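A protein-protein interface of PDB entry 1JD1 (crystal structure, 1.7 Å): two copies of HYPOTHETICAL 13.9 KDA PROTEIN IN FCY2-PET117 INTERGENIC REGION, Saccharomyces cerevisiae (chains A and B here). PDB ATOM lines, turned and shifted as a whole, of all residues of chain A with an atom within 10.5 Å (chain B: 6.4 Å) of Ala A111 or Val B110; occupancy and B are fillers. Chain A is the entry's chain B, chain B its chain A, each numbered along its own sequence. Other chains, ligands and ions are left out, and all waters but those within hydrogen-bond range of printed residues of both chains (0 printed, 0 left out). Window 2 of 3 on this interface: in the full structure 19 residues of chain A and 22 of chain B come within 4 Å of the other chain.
The backbone NH of Ala B109 sits at hydrogen-bond distance from the backbone carbonyl oxygen of Ala A112 (3.0 Å).
O of Ala B109 sits at hydrogen-bond distance from N of Ala A111, at 3.0 Å.
The backbone carbonyl oxygen (O) of Leu B81 is in hydrogen-bond range of the backbone NH (N) of Val B110 (2.7 Å).
The backbone carbonyl oxygen (O) of Glu A120 is in hydrogen-bond range of the backbone NH (N) of Phe A80.
O of Val B108 is in hydrogen-bond range of N of Leu B81.
The backbone carbonyl oxygen (O) of Leu A81 is in hydrogen-bond range of the backbone NH (N) of Val A110 (2.8 Å).
Among the printed residues, pairs that only touch across the chains: Phe A80 with Val B108 (3.7 Å), Val A110 with Ala B109 (3.2 Å), Ala A111 with Val B110 (3.6 Å), Ala A112 with Ile B84 (3.9 Å), Leu A113 with Ile B84 (3.7 Å), Leu A113 with Val B108 (3.7 Å), Pro A114 with Ile B84 (3.7 Å) and Glu A120 with Val B108 (3.5 Å).
Of the printed residues of chain B, Phe A80 touches Val B108 (3.7 Å).
Ala A111 touches two residues of chain B.
Of the printed residues of chain B, Pro A114 touches Ile B84 (3.7 Å).
Of the printed residues of chain B, Glu A120 touches Val B108 (3.5 Å).
No residue of chain A comes within 4 Å of Ala B82.
Of chain A, only Val A110 (3.2 Å), Ala A111 (3.0 Å) and Ala A112 (3.0 Å) come within 4 Å of Ala B109.
Val B110 touches just one residue of chain A: Ala A111.
Ala B112 touches none of the printed residues of chain A.
The nearest residue of chain A that does not touch Val B110 is Val A110 (4.6 Å).
The nearest printed residue of chain B that does not touch Leu A113 is Ala B109 (5.0 Å).
Of the 11 printed residues of chain B, 4 touch a printed residue of chain A.
Printed residues of chain B that touch a printed residue of chain A: Ile B84, Val B108, Ala B109 and Val B110.
Printed residues of chain A that touch a printed residue of chain B: Phe A80, Val A110, Ala A111, Ala A112, Leu A113, Pro A114 and Glu A120.
Hydrophobic or aromatic side chains of chain A within 4 Å of the printed part of chain B: Phe A80, Val A110, Ala A111, Ala A112 and Leu A113.
Phe A80 touches Val B108, but with the chains exchanged Val A108 does not touch Phe B80 (7.1 Å).
Ala A111 touches Val B110, but with the chains exchanged Val A110 does not touch Ala B111 (5.7 Å).
Ala A112 touches Ala B109, but with the chains exchanged Ala A109 does not touch Ala B112 (9.0 Å).
Leu A113 touches Val B108, but with the chains exchanged Val A108 does not touch Leu B113 (11.4 Å).
11 positions are printed for both chains.
Of the 10 pairs that touch across the chains among the printed residues, none has its exchanged pair printed and touching as well.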
ATOM      1  N   ILE A  79     -20.850 -20.645  16.159  1.00  0.00           N
ATOM      2  CA  ILE A  79     -20.160 -20.362  17.401  1.00  0.00           C
ATOM      3  C   ILE A  79     -21.151 -20.302  18.550  1.00  0.00           C
ATOM      4  O   ILE A  79     -22.203 -19.661  18.440  1.00  0.00           O
ATOM      5  CB  ILE A  79     -19.435 -18.970  17.360  1.00  0.00           C
ATOM      6  CG1 ILE A  79     -18.485 -18.897  16.161  1.00  0.00           C
ATOM      7  CG2 ILE A  79     -18.688 -18.732  18.664  1.00  0.00           C
ATOM      8  CD1 ILE A  79     -17.423 -19.975  16.120  1.00  0.00           C
ATOM      9  N   PHE A  80     -20.810 -20.955  19.652  1.00  0.00           N
ATOM     10  CA  PHE A  80     -21.640 -20.924  20.860  1.00  0.00           C
ATOM     11  C   PHE A  80     -20.732 -20.387  21.969  1.00  0.00           C
ATOM     12  O   PHE A  80     -19.712 -20.990  22.267  1.00  0.00           O
ATOM     13  CB  PHE A  80     -22.123 -22.332  21.214  1.00  0.00           C
ATOM     14  CG  PHE A  80     -22.930 -22.977  20.132  1.00  0.00           C
ATOM     15  CD1 PHE A  80     -22.348 -23.886  19.251  1.00  0.00           C
ATOM     16  CD2 PHE A  80     -24.281 -22.669  19.987  1.00  0.00           C
ATOM     17  CE1 PHE A  80     -23.097 -24.481  18.250  1.00  0.00           C
ATOM     18  CE2 PHE A  80     -25.040 -23.259  18.985  1.00  0.00           C
ATOM     19  CZ  PHE A  80     -24.444 -24.168  18.114  1.00  0.00           C
ATOM     20  N   LEU A  81     -21.102 -19.248  22.557  1.00  0.00           N
ATOM     21  CA  LEU A  81     -20.324 -18.613  23.622  1.00  0.00           C
ATOM     22  C   LEU A  81     -20.999 -18.801  24.976  1.00  0.00           C
ATOM     23  O   LEU A  81     -22.227 -18.783  25.072  1.00  0.00           O
ATOM     24  CB  LEU A  81     -20.193 -17.100  23.355  1.00  0.00           C
ATOM     25  CG  LEU A  81     -19.530 -16.671  22.046  1.00  0.00           C
ATOM     26  CD1 LEU A  81     -19.636 -15.141  21.903  1.00  0.00           C
ATOM     27  CD2 LEU A  81     -18.058 -17.138  22.031  1.00  0.00           C
ATOM     28  N   ALA A  82     -20.206 -18.943  26.036  1.00  0.00           N
ATOM     29  CA  ALA A  82     -20.790 -19.112  27.356  1.00  0.00           C
ATOM     30  C   ALA A  82     -21.182 -17.747  27.902  1.00  0.00           C
ATOM     31  O   ALA A  82     -21.972 -17.653  28.836  1.00  0.00           O
ATOM     32  CB  ALA A  82     -19.785 -19.795  28.308  1.00  0.00           C
ATOM     33  N   ASP A  83     -20.644 -16.691  27.297  1.00  0.00           N
ATOM     34  CA  ASP A  83     -20.910 -15.319  27.743  1.00  0.00           C
ATOM     35  C   ASP A  83     -20.832 -14.401  26.527  1.00  0.00           C
ATOM     36  O   ASP A  83     -19.786 -14.304  25.876  1.00  0.00           O
ATOM     37  CB  ASP A  83     -19.859 -14.926  28.799  1.00  0.00           C
ATOM     38  CG  ASP A  83     -20.077 -13.536  29.385  1.00  0.00           C
ATOM     39  OD1 ASP A  83     -19.438 -13.246  30.413  1.00  0.00           O
ATOM     40  OD2 ASP A  83     -20.862 -12.733  28.846  1.00  0.00           O
ATOM     41  N   ILE A  84     -21.945 -13.749  26.213  1.00  0.00           N
ATOM     42  CA  ILE A  84     -22.006 -12.862  25.057  1.00  0.00           C
ATOM     43  C   ILE A  84     -20.962 -11.742  25.106  1.00  0.00           C
ATOM     44  O   ILE A  84     -20.553 -11.223  24.059  1.00  0.00           O
ATOM     45  CB  ILE A  84     -23.437 -12.283  24.875  1.00  0.00           C
ATOM     46  CG1 ILE A  84     -23.571 -11.656  23.482  1.00  0.00           C
ATOM     47  CG2 ILE A  84     -23.744 -11.268  25.989  1.00  0.00           C
ATOM     48  CD1 ILE A  84     -23.524 -12.674  22.346  1.00  0.00           C
ATOM     49  N   VAL A 108     -24.164 -17.336  19.028  1.00  0.00           N
ATOM     50  CA  VAL A 108     -25.138 -17.134  20.092  1.00  0.00           C
ATOM     51  C   VAL A 108     -24.491 -17.434  21.423  1.00  0.00           C
ATOM     52  O   VAL A 108     -23.483 -18.151  21.488  1.00  0.00           O
ATOM     53  CB  VAL A 108     -26.353 -18.095  19.947  1.00  0.00           C
ATOM     54  CG1 VAL A 108     -27.002 -17.921  18.601  1.00  0.00           C
ATOM     55  CG2 VAL A 108     -25.903 -19.535  20.153  1.00  0.00           C
ATOM     56  N   ALA A 109     -25.050 -16.884  22.496  1.00  0.00           N
ATOM     57  CA  ALA A 109     -24.529 -17.149  23.829  1.00  0.00           C
ATOM     58  C   ALA A 109     -25.488 -18.150  24.433  1.00  0.00           C
ATOM     59  O   ALA A 109     -26.704 -17.933  24.442  1.00  0.00           O
ATOM     60  CB  ALA A 109     -24.495 -15.872  24.669  1.00  0.00           C
ATOM     61  N   VAL A 110     -24.951 -19.264  24.895  1.00  0.00           N
ATOM     62  CA  VAL A 110     -25.775 -20.296  25.495  1.00  0.00           C
ATOM     63  C   VAL A 110     -25.628 -20.276  27.009  1.00  0.00           C
ATOM     64  O   VAL A 110     -24.854 -19.499  27.572  1.00  0.00           O
ATOM     65  CB  VAL A 110     -25.388 -21.698  24.973  1.00  0.00           C
ATOM     66  CG1 VAL A 110     -25.661 -21.795  23.470  1.00  0.00           C
ATOM     67  CG2 VAL A 110     -23.929 -21.988  25.294  1.00  0.00           C
ATOM     68  N   ALA A 111     -26.357 -21.164  27.667  1.00  0.00           N
ATOM     69  CA  ALA A 111     -26.342 -21.251  29.120  1.00  0.00           C
ATOM     70  C   ALA A 111     -25.059 -21.866  29.663  1.00  0.00           C
ATOM     71  O   ALA A 111     -24.471 -21.366  30.615  1.00  0.00           O
ATOM     72  CB  ALA A 111     -27.545 -22.071  29.599  1.00  0.00           C
ATOM     73  N   ALA A 112     -24.634 -22.962  29.054  1.00  0.00           N
ATOM     74  CA  ALA A 112     -23.445 -23.650  29.519  1.00  0.00           C
ATOM     75  C   ALA A 112     -22.950 -24.582  28.436  1.00  0.00           C
ATOM     76  O   ALA A 112     -23.694 -24.949  27.522  1.00  0.00           O
ATOM     77  CB  ALA A 112     -23.764 -24.437  30.780  1.00  0.00           C
ATOM     78  N   LEU A 113     -21.677 -24.950  28.537  1.00  0.00           N
ATOM     79  CA  LEU A 113     -21.051 -25.835  27.572  1.00  0.00           C
ATOM     80  C   LEU A 113     -20.369 -26.982  28.306  1.00  0.00           C
ATOM     81  O   LEU A 113     -20.144 -26.908  29.520  1.00  0.00           O
ATOM     82  CB  LEU A 113     -20.001 -25.064  26.762  1.00  0.00           C
ATOM     83  CG  LEU A 113     -20.630 -23.935  25.951  1.00  0.00           C
ATOM     84  CD1 LEU A 113     -19.548 -23.017  25.396  1.00  0.00           C
ATOM     85  CD2 LEU A 113     -21.466 -24.544  24.819  1.00  0.00           C
ATOM     86  N   PRO A 114     -20.046 -28.065  27.581  1.00  0.00           N
ATOM     87  CA  PRO A 114     -19.383 -29.195  28.237  1.00  0.00           C
ATOM     88  C   PRO A 114     -18.121 -28.734  28.978  1.00  0.00           C
ATOM     89  O   PRO A 114     -17.414 -27.830  28.522  1.00  0.00           O
ATOM     90  CB  PRO A 114     -19.064 -30.116  27.070  1.00  0.00           C
ATOM     91  CG  PRO A 114     -20.228 -29.870  26.158  1.00  0.00           C
ATOM     92  CD  PRO A 114     -20.321 -28.373  26.164  1.00  0.00           C
ATOM     93  N   LEU A 115     -17.847 -29.365  30.117  1.00  0.00           N
ATOM     94  CA  LEU A 115     -16.675 -29.051  30.930  1.00  0.00           C
ATOM     95  C   LEU A 115     -16.594 -27.599  31.389  1.00  0.00           C
ATOM     96  O   LEU A 115     -15.538 -27.142  31.826  1.00  0.00           O
ATOM     97  CB  LEU A 115     -15.404 -29.439  30.166  1.00  0.00           C
ATOM     98  CG  LEU A 115     -15.277 -30.945  29.922  1.00  0.00           C
ATOM     99  CD1 LEU A 115     -14.024 -31.246  29.102  1.00  0.00           C
ATOM    100  CD2 LEU A 115     -15.207 -31.658  31.292  1.00  0.00           C
ATOM    101  N   GLY A 116     -17.710 -26.878  31.304  1.00  0.00           N
ATOM    102  CA  GLY A 116     -17.735 -25.485  31.720  1.00  0.00           C
ATOM    103  C   GLY A 116     -16.863 -24.551  30.893  1.00  0.00           C
ATOM    104  O   GLY A 116     -16.455 -23.487  31.380  1.00  0.00           O
ATOM    105  N   VAL A 117     -16.586 -24.913  29.642  1.00  0.00           N
ATOM    106  CA  VAL A 117     -15.739 -24.073  28.793  1.00  0.00           C
ATOM    107  C   VAL A 117     -16.415 -22.791  28.306  1.00  0.00           C
ATOM    108  O   VAL A 117     -17.635 -22.642  28.363  1.00  0.00           O
ATOM    109  CB  VAL A 117     -15.189 -24.845  27.552  1.00  0.00           C
ATOM    110  CG1 VAL A 117     -14.330 -26.023  28.005  1.00  0.00           C
ATOM    111  CG2 VAL A 117     -16.343 -25.323  26.664  1.00  0.00           C
ATOM    112  N   ASP A 118     -15.604 -21.865  27.810  1.00  0.00           N
ATOM    113  CA  ASP A 118     -16.097 -20.577  27.365  1.00  0.00           C
ATOM    114  C   ASP A 118     -16.707 -20.519  25.973  1.00  0.00           C
ATOM    115  O   ASP A 118     -17.450 -19.589  25.652  1.00  0.00           O
ATOM    116  CB  ASP A 118     -14.969 -19.565  27.498  1.00  0.00           C
ATOM    117  CG  ASP A 118     -14.666 -19.247  28.943  1.00  0.00           C
ATOM    118  OD1 ASP A 118     -13.495 -18.970  29.270  1.00  0.00           O
ATOM    119  OD2 ASP A 118     -15.614 -19.269  29.754  1.00  0.00           O
ATOM    120  N   MET A 119     -16.383 -21.494  25.133  1.00  0.00           N
ATOM    121  CA  MET A 119     -16.943 -21.513  23.795  1.00  0.00           C
ATOM    122  C   MET A 119     -16.864 -22.884  23.123  1.00  0.00           C
ATOM    123  O   MET A 119     -16.101 -23.758  23.543  1.00  0.00           O
ATOM    124  CB  MET A 119     -16.249 -20.438  22.925  1.00  0.00           C
ATOM    125  CG  MET A 119     -14.975 -20.871  22.220  1.00  0.00           C
ATOM    126  SD  MET A 119     -13.341 -20.384  22.904  1.00  0.00           S
ATOM    127  CE  MET A 119     -13.562 -18.695  23.564  1.00  0.00           C
ATOM    128  N   GLU A 120     -17.692 -23.073  22.102  1.00  0.00           N
ATOM    129  CA  GLU A 120     -17.706 -24.298  21.298  1.00  0.00           C
ATOM    130  C   GLU A 120     -17.938 -23.831  19.855  1.00  0.00           C
ATOM    131  O   GLU A 120     -18.809 -22.992  19.604  1.00  0.00           O
ATOM    132  CB  GLU A 120     -18.843 -25.242  21.734  1.00  0.00           C
ATOM    133  CG  GLU A 120     -18.854 -26.598  20.999  1.00  0.00           C
ATOM    134  CD  GLU A 120     -19.965 -27.517  21.499  1.00  0.00           C
ATOM    135  OE1 GLU A 120     -20.386 -27.336  22.649  1.00  0.00           O
ATOM    136  OE2 GLU A 120     -20.422 -28.415  20.762  1.00  0.00           O
ATOM    137  N   PHE B  80     -29.315 -30.072  22.049  1.00  0.00           N
ATOM    138  CA  PHE B  80     -29.554 -28.869  22.834  1.00  0.00           C
ATOM    139  C   PHE B  80     -30.137 -29.347  24.168  1.00  0.00           C
ATOM    140  O   PHE B  80     -31.229 -29.923  24.199  1.00  0.00           O
ATOM    141  CB  PHE B  80     -30.549 -27.950  22.120  1.00  0.00           C
ATOM    142  CG  PHE B  80     -30.083 -27.480  20.754  1.00  0.00           C
ATOM    143  CD1 PHE B  80     -30.573 -28.069  19.589  1.00  0.00           C
ATOM    144  CD2 PHE B  80     -29.150 -26.451  20.648  1.00  0.00           C
ATOM    145  CE1 PHE B  80     -30.149 -27.642  18.337  1.00  0.00           C
ATOM    146  CE2 PHE B  80     -28.711 -26.008  19.393  1.00  0.00           C
ATOM    147  CZ  PHE B  80     -29.211 -26.605  18.235  1.00  0.00           C
ATOM    148  N   LEU B  81     -29.419 -29.120  25.262  1.00  0.00           N
ATOM    149  CA  LEU B  81     -29.893 -29.553  26.578  1.00  0.00           C
ATOM    150  C   LEU B  81     -30.428 -28.383  27.376  1.00  0.00           C
ATOM    151  O   LEU B  81     -29.902 -27.271  27.292  1.00  0.00           O
ATOM    152  CB  LEU B  81     -28.751 -30.204  27.371  1.00  0.00           C
ATOM    153  CG  LEU B  81     -28.041 -31.399  26.737  1.00  0.00           C
ATOM    154  CD1 LEU B  81     -26.806 -31.753  27.590  1.00  0.00           C
ATOM    155  CD2 LEU B  81     -28.984 -32.599  26.652  1.00  0.00           C
ATOM    156  N   ALA B  82     -31.478 -28.621  28.153  1.00  0.00           N
ATOM    157  CA  ALA B  82     -32.019 -27.553  28.977  1.00  0.00           C
ATOM    158  C   ALA B  82     -31.150 -27.406  30.235  1.00  0.00           C
ATOM    159  O   ALA B  82     -31.194 -26.379  30.911  1.00  0.00           O
ATOM    160  CB  ALA B  82     -33.468 -27.866  29.366  1.00  0.00           C
ATOM    161  N   ASP B  83     -30.357 -28.436  30.521  1.00  0.00           N
ATOM    162  CA  ASP B  83     -29.461 -28.463  31.693  1.00  0.00           C
ATOM    163  C   ASP B  83     -28.162 -29.212  31.323  1.00  0.00           C
ATOM    164  O   ASP B  83     -28.194 -30.405  30.998  1.00  0.00           O
ATOM    165  CB  ASP B  83     -30.158 -29.191  32.847  1.00  0.00           C
ATOM    166  CG  ASP B  83     -29.441 -29.017  34.178  1.00  0.00           C
ATOM    167  OD1 ASP B  83     -28.210 -28.800  34.179  1.00  0.00           O
ATOM    168  OD2 ASP B  83     -30.112 -29.111  35.236  1.00  0.00           O
ATOM    169  N   ILE B  84     -27.023 -28.535  31.368  1.00  0.00           N
ATOM    170  CA  ILE B  84     -25.759 -29.202  31.012  1.00  0.00           C
ATOM    171  C   ILE B  84     -25.493 -30.412  31.905  1.00  0.00           C
ATOM    172  O   ILE B  84     -24.762 -31.331  31.522  1.00  0.00           O
ATOM    173  CB  ILE B  84     -24.549 -28.206  31.099  1.00  0.00           C
ATOM    174  CG1 ILE B  84     -23.300 -28.793  30.424  1.00  0.00           C
ATOM    175  CG2 ILE B  84     -24.270 -27.877  32.553  1.00  0.00           C
ATOM    176  CD1 ILE B  84     -23.415 -28.953  28.907  1.00  0.00           C
ATOM    177  N   VAL B 108     -24.781 -28.401  23.354  1.00  0.00           N
ATOM    178  CA  VAL B 108     -24.712 -27.194  24.160  1.00  0.00           C
ATOM    179  C   VAL B 108     -25.938 -27.200  25.063  1.00  0.00           C
ATOM    180  O   VAL B 108     -26.911 -27.926  24.803  1.00  0.00           O
ATOM    181  CB  VAL B 108     -24.746 -25.905  23.273  1.00  0.00           C
ATOM    182  CG1 VAL B 108     -23.630 -25.971  22.219  1.00  0.00           C
ATOM    183  CG2 VAL B 108     -26.118 -25.743  22.601  1.00  0.00           C
ATOM    184  N   ALA B 109     -25.878 -26.423  26.140  1.00  0.00           N
ATOM    185  CA  ALA B 109     -27.015 -26.316  27.042  1.00  0.00           C
ATOM    186  C   ALA B 109     -27.592 -24.937  26.790  1.00  0.00           C
ATOM    187  O   ALA B 109     -26.868 -23.935  26.765  1.00  0.00           O
ATOM    188  CB  ALA B 109     -26.581 -26.459  28.514  1.00  0.00           C
ATOM    189  N   VAL B 110     -28.898 -24.885  26.577  1.00  0.00           N
ATOM    190  CA  VAL B 110     -29.560 -23.617  26.313  1.00  0.00           C
ATOM    191  C   VAL B 110     -30.390 -23.179  27.504  1.00  0.00           C
ATOM    192  O   VAL B 110     -30.484 -23.899  28.503  1.00  0.00           O
ATOM    193  CB  VAL B 110     -30.458 -23.727  25.051  1.00  0.00           C
ATOM    194  CG1 VAL B 110     -29.602 -24.096  23.813  1.00  0.00           C
ATOM    195  CG2 VAL B 110     -31.538 -24.778  25.275  1.00  0.00           C
ATOM    196  N   ALA B 111     -31.002 -22.005  27.401  1.00  0.00           N
ATOM    197  CA  ALA B 111     -31.813 -21.490  28.500  1.00  0.00           C
ATOM    198  C   ALA B 111     -33.152 -22.206  28.669  1.00  0.00           C
ATOM    199  O   ALA B 111     -33.578 -22.462  29.801  1.00  0.00           O
ATOM    200  CB  ALA B 111     -32.043 -19.982  28.313  1.00  0.00           C
ATOM    201  N   ALA B 112     -33.818 -22.528  27.559  1.00  0.00           N
ATOM    202  CA  ALA B 112     -35.120 -23.198  27.622  1.00  0.00           C
ATOM    203  C   ALA B 112     -35.486 -23.755  26.253  1.00  0.00           C
ATOM    204  O   ALA B 112     -34.949 -23.312  25.237  1.00  0.00           O
ATOM    205  CB  ALA B 112     -36.198 -22.213  28.080  1.00  0.00           C
ATOM    206  N   LEU B 113     -36.395 -24.726  26.240  1.00  0.00           N
ATOM    207  CA  LEU B 113     -36.840 -25.359  25.009  1.00  0.00           C
ATOM    208  C   LEU B 113     -38.366 -25.348  24.910  1.00  0.00           C
ATOM    209  O   LEU B 113     -39.060 -25.175  25.918  1.00  0.00           O
ATOM    210  CB  LEU B 113     -36.322 -26.806  24.947  1.00  0.00           C
ATOM    211  CG  LEU B 113     -34.790 -26.977  24.944  1.00  0.00           C
ATOM    212  CD1 LEU B 113     -34.424 -28.436  25.207  1.00  0.00           C
ATOM    213  CD2 LEU B 113     -34.219 -26.505  23.602  1.00  0.00           C
